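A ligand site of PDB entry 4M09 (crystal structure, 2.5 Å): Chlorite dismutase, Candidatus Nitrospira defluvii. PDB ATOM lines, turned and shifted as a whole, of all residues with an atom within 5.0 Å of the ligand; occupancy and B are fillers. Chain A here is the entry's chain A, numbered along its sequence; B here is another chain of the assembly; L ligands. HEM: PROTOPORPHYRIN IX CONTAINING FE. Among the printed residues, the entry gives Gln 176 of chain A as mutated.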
ATOM      1  N   LYS A 110       1.598 -31.906 -23.601  1.00  0.00           N
ATOM      2  CA  LYS A 110       2.194 -32.502 -22.419  1.00  0.00           C
ATOM      3  C   LYS A 110       2.171 -31.471 -21.288  1.00  0.00           C
ATOM      4  O   LYS A 110       2.544 -30.315 -21.500  1.00  0.00           O
ATOM      5  CB  LYS A 110       3.617 -32.980 -22.681  1.00  0.00           C
ATOM      6  CG  LYS A 110       3.743 -34.027 -23.771  1.00  0.00           C
ATOM      7  CD  LYS A 110       5.216 -34.365 -24.026  1.00  0.00           C
ATOM      8  CE  LYS A 110       5.370 -35.408 -25.116  1.00  0.00           C
ATOM      9  NZ  LYS A 110       6.804 -35.733 -25.349  1.00  0.00           N
ATOM     10  N   PRO A 111       1.736 -31.890 -20.089  1.00  0.00           N
ATOM     11  CA  PRO A 111       1.583 -30.992 -18.929  1.00  0.00           C
ATOM     12  C   PRO A 111       2.809 -30.107 -18.715  1.00  0.00           C
ATOM     13  O   PRO A 111       3.934 -30.555 -18.910  1.00  0.00           O
ATOM     14  CB  PRO A 111       1.388 -31.968 -17.768  1.00  0.00           C
ATOM     15  CG  PRO A 111       0.726 -33.147 -18.384  1.00  0.00           C
ATOM     16  CD  PRO A 111       1.327 -33.271 -19.762  1.00  0.00           C
ATOM     17  N   THR A 112       2.581 -28.868 -18.294  1.00  0.00           N
ATOM     18  CA  THR A 112       3.665 -27.901 -18.146  1.00  0.00           C
ATOM     19  C   THR A 112       4.101 -27.727 -16.688  1.00  0.00           C
ATOM     20  O   THR A 112       5.281 -27.583 -16.392  1.00  0.00           O
ATOM     21  CB  THR A 112       3.272 -26.523 -18.722  1.00  0.00           C
ATOM     22  OG1 THR A 112       2.896 -26.672 -20.100  1.00  0.00           O
ATOM     23  CG2 THR A 112       4.424 -25.533 -18.615  1.00  0.00           C
ATOM     24  N   TYR A 113       3.130 -27.749 -15.776  1.00  0.00           N
ATOM     25  CA  TYR A 113       3.399 -27.425 -14.380  1.00  0.00           C
ATOM     26  C   TYR A 113       3.423 -28.647 -13.467  1.00  0.00           C
ATOM     27  O   TYR A 113       3.971 -28.588 -12.363  1.00  0.00           O
ATOM     28  CB  TYR A 113       2.345 -26.436 -13.860  1.00  0.00           C
ATOM     29  CG  TYR A 113       2.247 -25.152 -14.649  1.00  0.00           C
ATOM     30  CD1 TYR A 113       3.278 -24.217 -14.614  1.00  0.00           C
ATOM     31  CD2 TYR A 113       1.129 -24.874 -15.419  1.00  0.00           C
ATOM     32  CE1 TYR A 113       3.190 -23.037 -15.331  1.00  0.00           C
ATOM     33  CE2 TYR A 113       1.033 -23.694 -16.142  1.00  0.00           C
ATOM     34  CZ  TYR A 113       2.068 -22.780 -16.095  1.00  0.00           C
ATOM     35  OH  TYR A 113       1.967 -21.612 -16.812  1.00  0.00           O
ATOM     36  N   VAL A 114       2.856 -29.758 -13.931  1.00  0.00           N
ATOM     37  CA  VAL A 114       2.733 -30.958 -13.101  1.00  0.00           C
ATOM     38  C   VAL A 114       4.086 -31.487 -12.608  1.00  0.00           C
ATOM     39  O   VAL A 114       4.185 -31.978 -11.480  1.00  0.00           O
ATOM     40  CB  VAL A 114       1.997 -32.079 -13.877  1.00  0.00           C
ATOM     41  CG1 VAL A 114       1.915 -33.354 -13.051  1.00  0.00           C
ATOM     42  CG2 VAL A 114       0.613 -31.621 -14.274  1.00  0.00           C
ATOM     43  N   PHE A 117       5.256 -30.274  -9.232  1.00  0.00           N
ATOM     44  CA  PHE A 117       4.332 -30.502  -8.119  1.00  0.00           C
ATOM     45  C   PHE A 117       4.924 -31.475  -7.105  1.00  0.00           C
ATOM     46  O   PHE A 117       5.895 -32.166  -7.403  1.00  0.00           O
ATOM     47  CB  PHE A 117       2.992 -31.034  -8.639  1.00  0.00           C
ATOM     48  CG  PHE A 117       2.188 -30.035  -9.430  1.00  0.00           C
ATOM     49  CD1 PHE A 117       2.577 -28.710  -9.520  1.00  0.00           C
ATOM     50  CD2 PHE A 117       1.035 -30.428 -10.094  1.00  0.00           C
ATOM     51  CE1 PHE A 117       1.830 -27.798 -10.245  1.00  0.00           C
ATOM     52  CE2 PHE A 117       0.296 -29.524 -10.827  1.00  0.00           C
ATOM     53  CZ  PHE A 117       0.686 -28.210 -10.902  1.00  0.00           C
ATOM     54  N   LEU A 125      -3.229 -37.291  -9.111  1.00  0.00           N
ATOM     55  CA  LEU A 125      -3.628 -36.808 -10.421  1.00  0.00           C
ATOM     56  C   LEU A 125      -3.645 -37.943 -11.443  1.00  0.00           C
ATOM     57  O   LEU A 125      -4.323 -37.865 -12.475  1.00  0.00           O
ATOM     58  CB  LEU A 125      -2.688 -35.699 -10.894  1.00  0.00           C
ATOM     59  CG  LEU A 125      -2.880 -34.325 -10.240  1.00  0.00           C
ATOM     60  CD1 LEU A 125      -1.927 -33.299 -10.831  1.00  0.00           C
ATOM     61  CD2 LEU A 125      -4.328 -33.869 -10.403  1.00  0.00           C
ATOM     62  N   ILE A 140     -15.850 -25.079 -21.192  1.00  0.00           N
ATOM     63  CA  ILE A 140     -15.592 -23.700 -20.803  1.00  0.00           C
ATOM     64  C   ILE A 140     -14.283 -23.194 -21.395  1.00  0.00           C
ATOM     65  O   ILE A 140     -13.206 -23.659 -21.031  1.00  0.00           O
ATOM     66  CB  ILE A 140     -15.533 -23.539 -19.265  1.00  0.00           C
ATOM     67  CG1 ILE A 140     -16.886 -23.902 -18.644  1.00  0.00           C
ATOM     68  CG2 ILE A 140     -15.161 -22.110 -18.896  1.00  0.00           C
ATOM     69  CD1 ILE A 140     -16.878 -23.870 -17.127  1.00  0.00           C
ATOM     70  N   ILE A 142     -11.362 -20.328 -21.848  1.00  0.00           N
ATOM     71  CA  ILE A 142     -10.760 -19.442 -20.857  1.00  0.00           C
ATOM     72  C   ILE A 142      -9.649 -18.602 -21.473  1.00  0.00           C
ATOM     73  O   ILE A 142      -8.831 -19.099 -22.249  1.00  0.00           O
ATOM     74  CB  ILE A 142     -10.223 -20.253 -19.650  1.00  0.00           C
ATOM     75  CG1 ILE A 142     -11.374 -20.718 -18.767  1.00  0.00           C
ATOM     76  CG2 ILE A 142      -9.254 -19.421 -18.821  1.00  0.00           C
ATOM     77  CD1 ILE A 142     -10.962 -21.596 -17.612  1.00  0.00           C
ATOM     78  N   LYS A 144      -6.593 -15.870 -20.334  1.00  0.00           N
ATOM     79  CA  LYS A 144      -5.807 -15.285 -19.254  1.00  0.00           C
ATOM     80  C   LYS A 144      -5.506 -13.811 -19.540  1.00  0.00           C
ATOM     81  O   LYS A 144      -5.383 -13.415 -20.696  1.00  0.00           O
ATOM     82  CB  LYS A 144      -4.508 -16.061 -19.049  1.00  0.00           C
ATOM     83  CG  LYS A 144      -4.715 -17.496 -18.620  1.00  0.00           C
ATOM     84  CD  LYS A 144      -5.307 -17.565 -17.217  1.00  0.00           C
ATOM     85  CE  LYS A 144      -5.184 -18.957 -16.626  1.00  0.00           C
ATOM     86  NZ  LYS A 144      -5.926 -19.074 -15.337  1.00  0.00           N
ATOM     87  N   TRP A 148      -0.917 -12.481 -16.241  1.00  0.00           N
ATOM     88  CA  TRP A 148      -0.583 -13.897 -16.070  1.00  0.00           C
ATOM     89  C   TRP A 148       0.670 -14.334 -16.831  1.00  0.00           C
ATOM     90  O   TRP A 148       1.508 -15.050 -16.302  1.00  0.00           O
ATOM     91  CB  TRP A 148      -1.758 -14.783 -16.490  1.00  0.00           C
ATOM     92  CG  TRP A 148      -1.376 -16.221 -16.702  1.00  0.00           C
ATOM     93  CD1 TRP A 148      -1.002 -16.808 -17.876  1.00  0.00           C
ATOM     94  CD2 TRP A 148      -1.299 -17.246 -15.709  1.00  0.00           C
ATOM     95  NE1 TRP A 148      -0.718 -18.132 -17.678  1.00  0.00           N
ATOM     96  CE2 TRP A 148      -0.885 -18.434 -16.348  1.00  0.00           C
ATOM     97  CE3 TRP A 148      -1.544 -17.288 -14.328  1.00  0.00           C
ATOM     98  CZ2 TRP A 148      -0.716 -19.629 -15.668  1.00  0.00           C
ATOM     99  CZ3 TRP A 148      -1.374 -18.484 -13.649  1.00  0.00           C
ATOM    100  CH2 TRP A 148      -0.966 -19.640 -14.328  1.00  0.00           C
ATOM    101  N   MET A 160      -0.735 -22.704 -10.015  1.00  0.00           N
ATOM    102  CA  MET A 160      -1.425 -23.850 -10.580  1.00  0.00           C
ATOM    103  C   MET A 160      -1.468 -25.015  -9.593  1.00  0.00           C
ATOM    104  O   MET A 160      -2.337 -25.889  -9.696  1.00  0.00           O
ATOM    105  CB  MET A 160      -0.781 -24.284 -11.896  1.00  0.00           C
ATOM    106  CG  MET A 160      -0.914 -23.272 -13.018  1.00  0.00           C
ATOM    107  SD  MET A 160      -2.593 -22.628 -13.226  1.00  0.00           S
ATOM    108  CE  MET A 160      -3.525 -24.133 -13.482  1.00  0.00           C
ATOM    109  N   HIS A 163      -4.285 -24.162  -7.643  1.00  0.00           N
ATOM    110  CA  HIS A 163      -5.386 -24.525  -8.518  1.00  0.00           C
ATOM    111  C   HIS A 163      -5.706 -26.013  -8.395  1.00  0.00           C
ATOM    112  O   HIS A 163      -6.834 -26.394  -8.081  1.00  0.00           O
ATOM    113  CB  HIS A 163      -5.048 -24.170  -9.967  1.00  0.00           C
ATOM    114  CG  HIS A 163      -6.066 -24.646 -10.955  1.00  0.00           C
ATOM    115  ND1 HIS A 163      -7.050 -23.823 -11.464  1.00  0.00           N
ATOM    116  CD2 HIS A 163      -6.238 -25.848 -11.548  1.00  0.00           C
ATOM    117  CE1 HIS A 163      -7.792 -24.505 -12.308  1.00  0.00           C
ATOM    118  NE2 HIS A 163      -7.321 -25.745 -12.377  1.00  0.00           N
ATOM    119  N   THR A 164      -4.699 -26.842  -8.644  1.00  0.00           N
ATOM    120  CA  THR A 164      -4.845 -28.298  -8.599  1.00  0.00           C
ATOM    121  C   THR A 164      -5.298 -28.779  -7.233  1.00  0.00           C
ATOM    122  O   THR A 164      -6.101 -29.715  -7.127  1.00  0.00           O
ATOM    123  CB  THR A 164      -3.528 -29.000  -8.972  1.00  0.00           C
ATOM    124  OG1 THR A 164      -3.035 -28.499 -10.224  1.00  0.00           O
ATOM    125  CG2 THR A 164      -3.731 -30.507  -9.092  1.00  0.00           C
ATOM    126  N   ALA A 167      -8.936 -28.696  -6.620  1.00  0.00           N
ATOM    127  CA  ALA A 167      -9.666 -29.544  -7.559  1.00  0.00           C
ATOM    128  C   ALA A 167      -9.607 -31.024  -7.205  1.00  0.00           C
ATOM    129  O   ALA A 167     -10.493 -31.796  -7.557  1.00  0.00           O
ATOM    130  CB  ALA A 167      -9.134 -29.322  -8.974  1.00  0.00           C
ATOM    131  N   TYR A 170     -12.361 -33.681  -6.374  1.00  0.00           N
ATOM    132  CA  TYR A 170     -13.425 -33.830  -7.351  1.00  0.00           C
ATOM    133  C   TYR A 170     -13.007 -34.777  -8.487  1.00  0.00           C
ATOM    134  O   TYR A 170     -13.782 -35.035  -9.401  1.00  0.00           O
ATOM    135  CB  TYR A 170     -13.822 -32.473  -7.935  1.00  0.00           C
ATOM    136  CG  TYR A 170     -14.424 -31.539  -6.912  1.00  0.00           C
ATOM    137  CD1 TYR A 170     -15.795 -31.476  -6.714  1.00  0.00           C
ATOM    138  CD2 TYR A 170     -13.612 -30.710  -6.138  1.00  0.00           C
ATOM    139  CE1 TYR A 170     -16.341 -30.619  -5.780  1.00  0.00           C
ATOM    140  CE2 TYR A 170     -14.151 -29.852  -5.211  1.00  0.00           C
ATOM    141  CZ  TYR A 170     -15.519 -29.808  -5.028  1.00  0.00           C
ATOM    142  OH  TYR A 170     -16.059 -28.950  -4.101  1.00  0.00           O
ATOM    143  N   LEU A 171     -11.775 -35.274  -8.388  1.00  0.00           N
ATOM    144  CA  LEU A 171     -11.222 -36.166  -9.395  1.00  0.00           C
ATOM    145  C   LEU A 171     -12.050 -37.436  -9.554  1.00  0.00           C
ATOM    146  O   LEU A 171     -12.161 -37.984 -10.644  1.00  0.00           O
ATOM    147  CB  LEU A 171      -9.775 -36.531  -9.028  1.00  0.00           C
ATOM    148  CG  LEU A 171      -8.698 -35.740  -9.788  1.00  0.00           C
ATOM    149  CD1 LEU A 171      -7.311 -36.131  -9.302  1.00  0.00           C
ATOM    150  CD2 LEU A 171      -8.819 -35.963 -11.286  1.00  0.00           C
ATOM    151  N   VAL A 174     -15.511 -36.120 -11.371  1.00  0.00           N
ATOM    152  CA  VAL A 174     -15.457 -35.247 -12.536  1.00  0.00           C
ATOM    153  C   VAL A 174     -14.223 -35.520 -13.396  1.00  0.00           C
ATOM    154  O   VAL A 174     -13.094 -35.332 -12.955  1.00  0.00           O
ATOM    155  CB  VAL A 174     -15.439 -33.755 -12.133  1.00  0.00           C
ATOM    156  CG1 VAL A 174     -15.219 -32.883 -13.363  1.00  0.00           C
ATOM    157  CG2 VAL A 174     -16.738 -33.382 -11.431  1.00  0.00           C
ATOM    158  N   GLN A 176     -11.747 -34.603 -16.468  1.00  0.00           N
ATOM    159  CA  GLN A 176     -11.319 -33.337 -17.042  1.00  0.00           C
ATOM    160  C   GLN A 176     -10.245 -33.513 -18.107  1.00  0.00           C
ATOM    161  O   GLN A 176      -9.419 -34.420 -18.027  1.00  0.00           O
ATOM    162  CB  GLN A 176     -10.836 -32.386 -15.941  1.00  0.00           C
ATOM    163  CG  GLN A 176      -9.961 -33.022 -14.876  1.00  0.00           C
ATOM    164  CD  GLN A 176      -8.535 -33.245 -15.338  1.00  0.00           C
ATOM    165  OE1 GLN A 176      -8.026 -32.529 -16.203  1.00  0.00           O
ATOM    166  NE2 GLN A 176      -7.879 -34.256 -14.765  1.00  0.00           N
ATOM    167  N   LEU A 178      -7.822 -30.879 -21.026  1.00  0.00           N
ATOM    168  CA  LEU A 178      -7.469 -29.506 -21.367  1.00  0.00           C
ATOM    169  C   LEU A 178      -6.913 -29.391 -22.781  1.00  0.00           C
ATOM    170  O   LEU A 178      -6.075 -30.197 -23.205  1.00  0.00           O
ATOM    171  CB  LEU A 178      -6.456 -28.951 -20.354  1.00  0.00           C
ATOM    172  CG  LEU A 178      -5.806 -27.603 -20.664  1.00  0.00           C
ATOM    173  CD1 LEU A 178      -6.825 -26.474 -20.562  1.00  0.00           C
ATOM    174  CD2 LEU A 178      -4.629 -27.352 -19.739  1.00  0.00           C
ATOM    175  N   PHE A 189      -7.496 -21.295 -23.812  1.00  0.00           N
ATOM    176  CA  PHE A 189      -7.712 -22.672 -23.379  1.00  0.00           C
ATOM    177  C   PHE A 189      -9.135 -23.130 -23.626  1.00  0.00           C
ATOM    178  O   PHE A 189     -10.060 -22.320 -23.725  1.00  0.00           O
ATOM    179  CB  PHE A 189      -7.388 -22.822 -21.888  1.00  0.00           C
ATOM    180  CG  PHE A 189      -5.961 -22.480 -21.534  1.00  0.00           C
ATOM    181  CD1 PHE A 189      -4.982 -23.447 -21.557  1.00  0.00           C
ATOM    182  CD2 PHE A 189      -5.624 -21.188 -21.158  1.00  0.00           C
ATOM    183  CE1 PHE A 189      -3.678 -23.143 -21.232  1.00  0.00           C
ATOM    184  CE2 PHE A 189      -4.321 -20.875 -20.832  1.00  0.00           C
ATOM    185  CZ  PHE A 189      -3.348 -21.853 -20.863  1.00  0.00           C
ATOM    186  N   THR A 191     -11.631 -26.061 -21.835  1.00  0.00           N
ATOM    187  CA  THR A 191     -11.745 -27.049 -20.781  1.00  0.00           C
ATOM    188  C   THR A 191     -12.974 -27.914 -21.008  1.00  0.00           C
ATOM    189  O   THR A 191     -14.049 -27.419 -21.349  1.00  0.00           O
ATOM    190  CB  THR A 191     -11.823 -26.396 -19.387  1.00  0.00           C
ATOM    191  OG1 THR A 191     -12.940 -25.503 -19.331  1.00  0.00           O
ATOM    192  CG2 THR A 191     -10.544 -25.618 -19.101  1.00  0.00           C
ATOM    193  N   PHE A 193     -15.335 -31.286 -19.460  1.00  0.00           N
ATOM    194  CA  PHE A 193     -15.626 -32.066 -18.267  1.00  0.00           C
ATOM    195  C   PHE A 193     -16.788 -33.034 -18.465  1.00  0.00           C
ATOM    196  O   PHE A 193     -17.779 -32.702 -19.112  1.00  0.00           O
ATOM    197  CB  PHE A 193     -15.932 -31.145 -17.083  1.00  0.00           C
ATOM    198  CG  PHE A 193     -14.885 -30.086 -16.866  1.00  0.00           C
ATOM    199  CD1 PHE A 193     -13.729 -30.374 -16.160  1.00  0.00           C
ATOM    200  CD2 PHE A 193     -15.068 -28.811 -17.357  1.00  0.00           C
ATOM    201  CE1 PHE A 193     -12.767 -29.409 -15.961  1.00  0.00           C
ATOM    202  CE2 PHE A 193     -14.107 -27.835 -17.158  1.00  0.00           C
ATOM    203  CZ  PHE A 193     -12.957 -28.134 -16.460  1.00  0.00           C
ATOM    204  N   PHE A 201     -19.778 -30.734  -9.775  1.00  0.00           N
ATOM    205  CA  PHE A 201     -19.102 -29.854 -10.725  1.00  0.00           C
ATOM    206  C   PHE A 201     -19.257 -28.400 -10.315  1.00  0.00           C
ATOM    207  O   PHE A 201     -18.348 -27.595 -10.513  1.00  0.00           O
ATOM    208  CB  PHE A 201     -19.640 -30.067 -12.148  1.00  0.00           C
ATOM    209  CG  PHE A 201     -18.970 -29.195 -13.177  1.00  0.00           C
ATOM    210  CD1 PHE A 201     -17.686 -29.473 -13.605  1.00  0.00           C
ATOM    211  CD2 PHE A 201     -19.633 -28.096 -13.709  1.00  0.00           C
ATOM    212  CE1 PHE A 201     -17.067 -28.683 -14.560  1.00  0.00           C
ATOM    213  CE2 PHE A 201     -19.022 -27.298 -14.656  1.00  0.00           C
ATOM    214  CZ  PHE A 201     -17.735 -27.596 -15.085  1.00  0.00           C
ATOM    215  N   LEU A 204     -17.061 -27.778  -7.389  1.00  0.00           N
ATOM    216  CA  LEU A 204     -15.731 -27.757  -7.964  1.00  0.00           C
ATOM    217  C   LEU A 204     -15.339 -26.360  -8.446  1.00  0.00           C
ATOM    218  O   LEU A 204     -14.199 -25.924  -8.241  1.00  0.00           O
ATOM    219  CB  LEU A 204     -15.652 -28.737  -9.128  1.00  0.00           C
ATOM    220  CG  LEU A 204     -14.465 -28.586 -10.085  1.00  0.00           C
ATOM    221  CD1 LEU A 204     -13.171 -29.023  -9.417  1.00  0.00           C
ATOM    222  CD2 LEU A 204     -14.719 -29.360 -11.363  1.00  0.00           C
ATOM    223  N   VAL A 205     -16.281 -25.667  -9.068  1.00  0.00           N
ATOM    224  CA  VAL A 205     -15.987 -24.370  -9.682  1.00  0.00           C
ATOM    225  C   VAL A 205     -15.824 -23.252  -8.662  1.00  0.00           C
ATOM    226  O   VAL A 205     -14.893 -22.448  -8.769  1.00  0.00           O
ATOM    227  CB  VAL A 205     -17.074 -23.972 -10.708  1.00  0.00           C
ATOM    228  CG1 VAL A 205     -16.771 -22.603 -11.298  1.00  0.00           C
ATOM    229  CG2 VAL A 205     -17.150 -25.009 -11.824  1.00  0.00           C
ATOM    230  N   LEU A 208     -12.609 -23.347  -7.098  1.00  0.00           N
ATOM    231  CA  LEU A 208     -11.569 -22.770  -7.940  1.00  0.00           C
ATOM    232  C   LEU A 208     -11.752 -21.269  -8.101  1.00  0.00           C
ATOM    233  O   LEU A 208     -10.894 -20.594  -8.674  1.00  0.00           O
ATOM    234  CB  LEU A 208     -11.551 -23.455  -9.300  1.00  0.00           C
ATOM    235  CG  LEU A 208     -10.736 -24.741  -9.352  1.00  0.00           C
ATOM    236  CD1 LEU A 208     -10.841 -25.415 -10.718  1.00  0.00           C
ATOM    237  CD2 LEU A 208      -9.285 -24.456  -9.001  1.00  0.00           C
ATOM    238  N   GLU A 213      -5.478 -17.654  -8.886  1.00  0.00           N
ATOM    239  CA  GLU A 213      -5.345 -17.809 -10.333  1.00  0.00           C
ATOM    240  C   GLU A 213      -6.566 -17.246 -11.045  1.00  0.00           C
ATOM    241  O   GLU A 213      -6.460 -16.654 -12.119  1.00  0.00           O
ATOM    242  CB  GLU A 213      -5.145 -19.279 -10.688  1.00  0.00           C
ATOM    243  CG  GLU A 213      -5.181 -19.580 -12.176  1.00  0.00           C
ATOM    244  CD  GLU A 213      -5.726 -20.960 -12.478  1.00  0.00           C
ATOM    245  OE1 GLU A 213      -6.215 -21.616 -11.538  1.00  0.00           O
ATOM    246  OE2 GLU A 213      -5.664 -21.384 -13.655  1.00  0.00           O
ATOM    247  N   PHE A 220     -14.207 -15.739 -18.909  1.00  0.00           N
ATOM    248  CA  PHE A 220     -14.557 -16.996 -18.257  1.00  0.00           C
ATOM    249  C   PHE A 220     -15.922 -17.455 -18.717  1.00  0.00           C
ATOM    250  O   PHE A 220     -16.950 -16.944 -18.272  1.00  0.00           O
ATOM    251  CB  PHE A 220     -14.524 -16.850 -16.735  1.00  0.00           C
ATOM    252  CG  PHE A 220     -14.573 -18.155 -15.995  1.00  0.00           C
ATOM    253  CD1 PHE A 220     -13.448 -18.962 -15.926  1.00  0.00           C
ATOM    254  CD2 PHE A 220     -15.745 -18.578 -15.393  1.00  0.00           C
ATOM    255  CE1 PHE A 220     -13.491 -20.171 -15.260  1.00  0.00           C
ATOM    256  CE2 PHE A 220     -15.788 -19.788 -14.712  1.00  0.00           C
ATOM    257  CZ  PHE A 220     -14.657 -20.583 -14.649  1.00  0.00           C
ATOM    258  N   ARG B 206       2.223 -17.841 -27.740  1.00  0.00           N
ATOM    259  CA  ARG B 206       2.413 -17.787 -26.295  1.00  0.00           C
ATOM    260  C   ARG B 206       3.795 -17.248 -25.958  1.00  0.00           C
ATOM    261  O   ARG B 206       3.998 -16.643 -24.908  1.00  0.00           O
ATOM    262  CB  ARG B 206       2.189 -19.156 -25.642  1.00  0.00           C
ATOM    263  CG  ARG B 206       2.147 -19.082 -24.109  1.00  0.00           C
ATOM    264  CD  ARG B 206       1.716 -20.374 -23.444  1.00  0.00           C
ATOM    265  NE  ARG B 206       1.408 -20.154 -22.028  1.00  0.00           N
ATOM    266  CZ  ARG B 206       0.986 -21.099 -21.182  1.00  0.00           C
ATOM    267  NH1 ARG B 206       0.820 -22.340 -21.607  1.00  0.00           N
ATOM    268  NH2 ARG B 206       0.735 -20.791 -19.918  1.00  0.00           N
HETATM  269  CHA HEM L   1      -4.558 -26.475 -15.828  1.00  0.00           C
HETATM  270  CHB HEM L   1      -5.975 -29.980 -12.771  1.00  0.00           C
HETATM  271  CHC HEM L   1     -10.595 -28.497 -13.027  1.00  0.00           C
HETATM  272  CHD HEM L   1      -9.147 -24.704 -15.693  1.00  0.00           C
HETATM  273  C1A HEM L   1      -4.529 -27.551 -14.964  1.00  0.00           C
HETATM  274  C2A HEM L   1      -3.356 -28.308 -14.552  1.00  0.00           C
HETATM  275  C3A HEM L   1      -3.754 -29.269 -13.714  1.00  0.00           C
HETATM  276  C4A HEM L   1      -5.189 -29.163 -13.556  1.00  0.00           C
HETATM  277  CMA HEM L   1      -2.843 -30.305 -13.025  1.00  0.00           C
HETATM  278  CAA HEM L   1      -1.888 -28.080 -14.976  1.00  0.00           C
HETATM  279  CBA HEM L   1      -1.713 -28.133 -16.488  1.00  0.00           C
HETATM  280  CGA HEM L   1      -0.251 -28.318 -16.792  1.00  0.00           C
HETATM  281  O1A HEM L   1       0.508 -28.722 -15.877  1.00  0.00           O
HETATM  282  O2A HEM L   1       0.154 -28.069 -17.958  1.00  0.00           O
HETATM  283  C1B HEM L   1      -7.349 -29.943 -12.667  1.00  0.00           C
HETATM  284  C2B HEM L   1      -8.177 -30.988 -12.100  1.00  0.00           C
HETATM  285  C3B HEM L   1      -9.448 -30.611 -12.162  1.00  0.00           C
HETATM  286  C4B HEM L   1      -9.489 -29.277 -12.772  1.00  0.00           C
HETATM  287  CMB HEM L   1      -7.660 -32.335 -11.537  1.00  0.00           C
HETATM  288  CAB HEM L   1     -10.620 -31.475 -11.653  1.00  0.00           C
HETATM  289  CBB HEM L   1     -11.895 -31.162 -11.861  1.00  0.00           C
HETATM  290  C1C HEM L   1     -10.593 -27.303 -13.722  1.00  0.00           C
HETATM  291  C2C HEM L   1     -11.732 -26.412 -13.900  1.00  0.00           C
HETATM  292  C3C HEM L   1     -11.326 -25.364 -14.642  1.00  0.00           C
HETATM  293  C4C HEM L   1      -9.927 -25.558 -14.953  1.00  0.00           C
HETATM  294  CMC HEM L   1     -13.134 -26.689 -13.309  1.00  0.00           C
HETATM  295  CAC HEM L   1     -12.120 -24.116 -15.130  1.00  0.00           C
HETATM  296  CBC HEM L   1     -13.418 -23.889 -14.924  1.00  0.00           C
HETATM  297  C1D HEM L   1      -7.806 -24.845 -16.036  1.00  0.00           C
HETATM  298  C2D HEM L   1      -7.096 -24.001 -16.975  1.00  0.00           C
HETATM  299  C3D HEM L   1      -5.663 -24.540 -17.014  1.00  0.00           C
HETATM  300  C4D HEM L   1      -5.654 -25.672 -16.110  1.00  0.00           C
HETATM  301  CMD HEM L   1      -7.647 -22.790 -17.757  1.00  0.00           C
HETATM  302  CAD HEM L   1      -4.522 -23.966 -17.884  1.00  0.00           C
HETATM  303  CBD HEM L   1      -3.290 -23.619 -17.054  1.00  0.00           C
HETATM  304  CGD HEM L   1      -2.660 -22.363 -17.602  1.00  0.00           C
HETATM  305  O1D HEM L   1      -1.439 -22.384 -17.910  1.00  0.00           O
HETATM  306  O2D HEM L   1      -3.382 -21.346 -17.742  1.00  0.00           O
HETATM  307  NA  HEM L   1      -5.623 -28.105 -14.340  1.00  0.00           N
HETATM  308  NB  HEM L   1      -8.179 -28.918 -13.067  1.00  0.00           N
HETATM  309  NC  HEM L   1      -9.514 -26.750 -14.374  1.00  0.00           N
HETATM  310  ND  HEM L   1      -6.927 -25.815 -15.563  1.00  0.00           N
HETATM  311 FE   HEM L   1      -7.567 -27.412 -14.360  1.00  0.00          FE
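An oxygen (O2A) of the ligand sits at hydrogen-bond distance from the backbone NH (N) of Thr 112.
N of Tyr 113 lies within hydrogen-bond range of O1A of the ligand (2.8 Å).
An oxygen (O1A) of the ligand lies within hydrogen-bond range of the backbone NH of Val 114 (3.2 Å).
An oxygen (O1D) of the ligand is in salt-bridge range of the guanidinium group (NH2) of Arg 206 of chain B, at 3.4 Å.
The side-chain hydroxyl (OH) of Tyr 113 sits at hydrogen-bond distance from the guanidinium group (NH2) of Arg 206 of chain B (3.4 Å).
The backbone carbonyl oxygen of Ile 142 lies within hydrogen-bond range of the backbone NH of Phe 189, at 3.0 Å.
The side-chain amino group (NZ) of Lys 144 lies within salt-bridge range of the side-chain carboxylate (OE2) of Glu 213, at 2.9 Å.
The backbone carbonyl oxygen (O) of Met 160 sits at hydrogen-bond distance from the side-chain hydroxyl (OG1) of Thr 164, 2.8 Å away.
The side-chain hydroxyl of Thr 191 is in hydrogen-bond range of the backbone carbonyl oxygen of Ile 140 (2.5 Å).
NC of the ligand sits close to NE2 of His 163 (3.1 Å).
Pro 111 touches the ligand.
Phe 117 touches the ligand.
Leu 125 touches the ligand.
Ile 142 touches the ligand.
Lys 144 touches the ligand.
CZ2 of Trp 148 touches O1D of the ligand (3.6 Å).
CE of Met 160 touches CHA of the ligand (3.5 Å).
OG1 of Thr 164 touches CMA of the ligand, 3.3 Å away.
CB of Ala 167 touches C3B of the ligand (3.5 Å).
Leu 171 touches the ligand (CD2 to CMB, 3.8 Å).
CG of Gln 176 touches CAB of the ligand, 3.6 Å away.
CD2 of Leu 178 touches CAD of the ligand, 3.9 Å away.
CZ of Phe 189 touches O2D of the ligand, 3.2 Å away.
Thr 191 touches the ligand.
Phe 193 touches the ligand (CZ to C2C, 3.3 Å).
CD2 of Leu 204 touches CBB of the ligand (3.4 Å).
Leu 208 touches the ligand (CD1 to C2C, 3.5 Å).
CZ of Phe 220 touches CBC of the ligand, 3.5 Å away.
Of the 30 residues printed, 23 come within 4 Å of the ligand.
Along chain A the residues within 4 Å of the ligand span positions 111 to 220.
The nearest printed residue that does not touch the ligand is Val 174 (4.03 Å).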
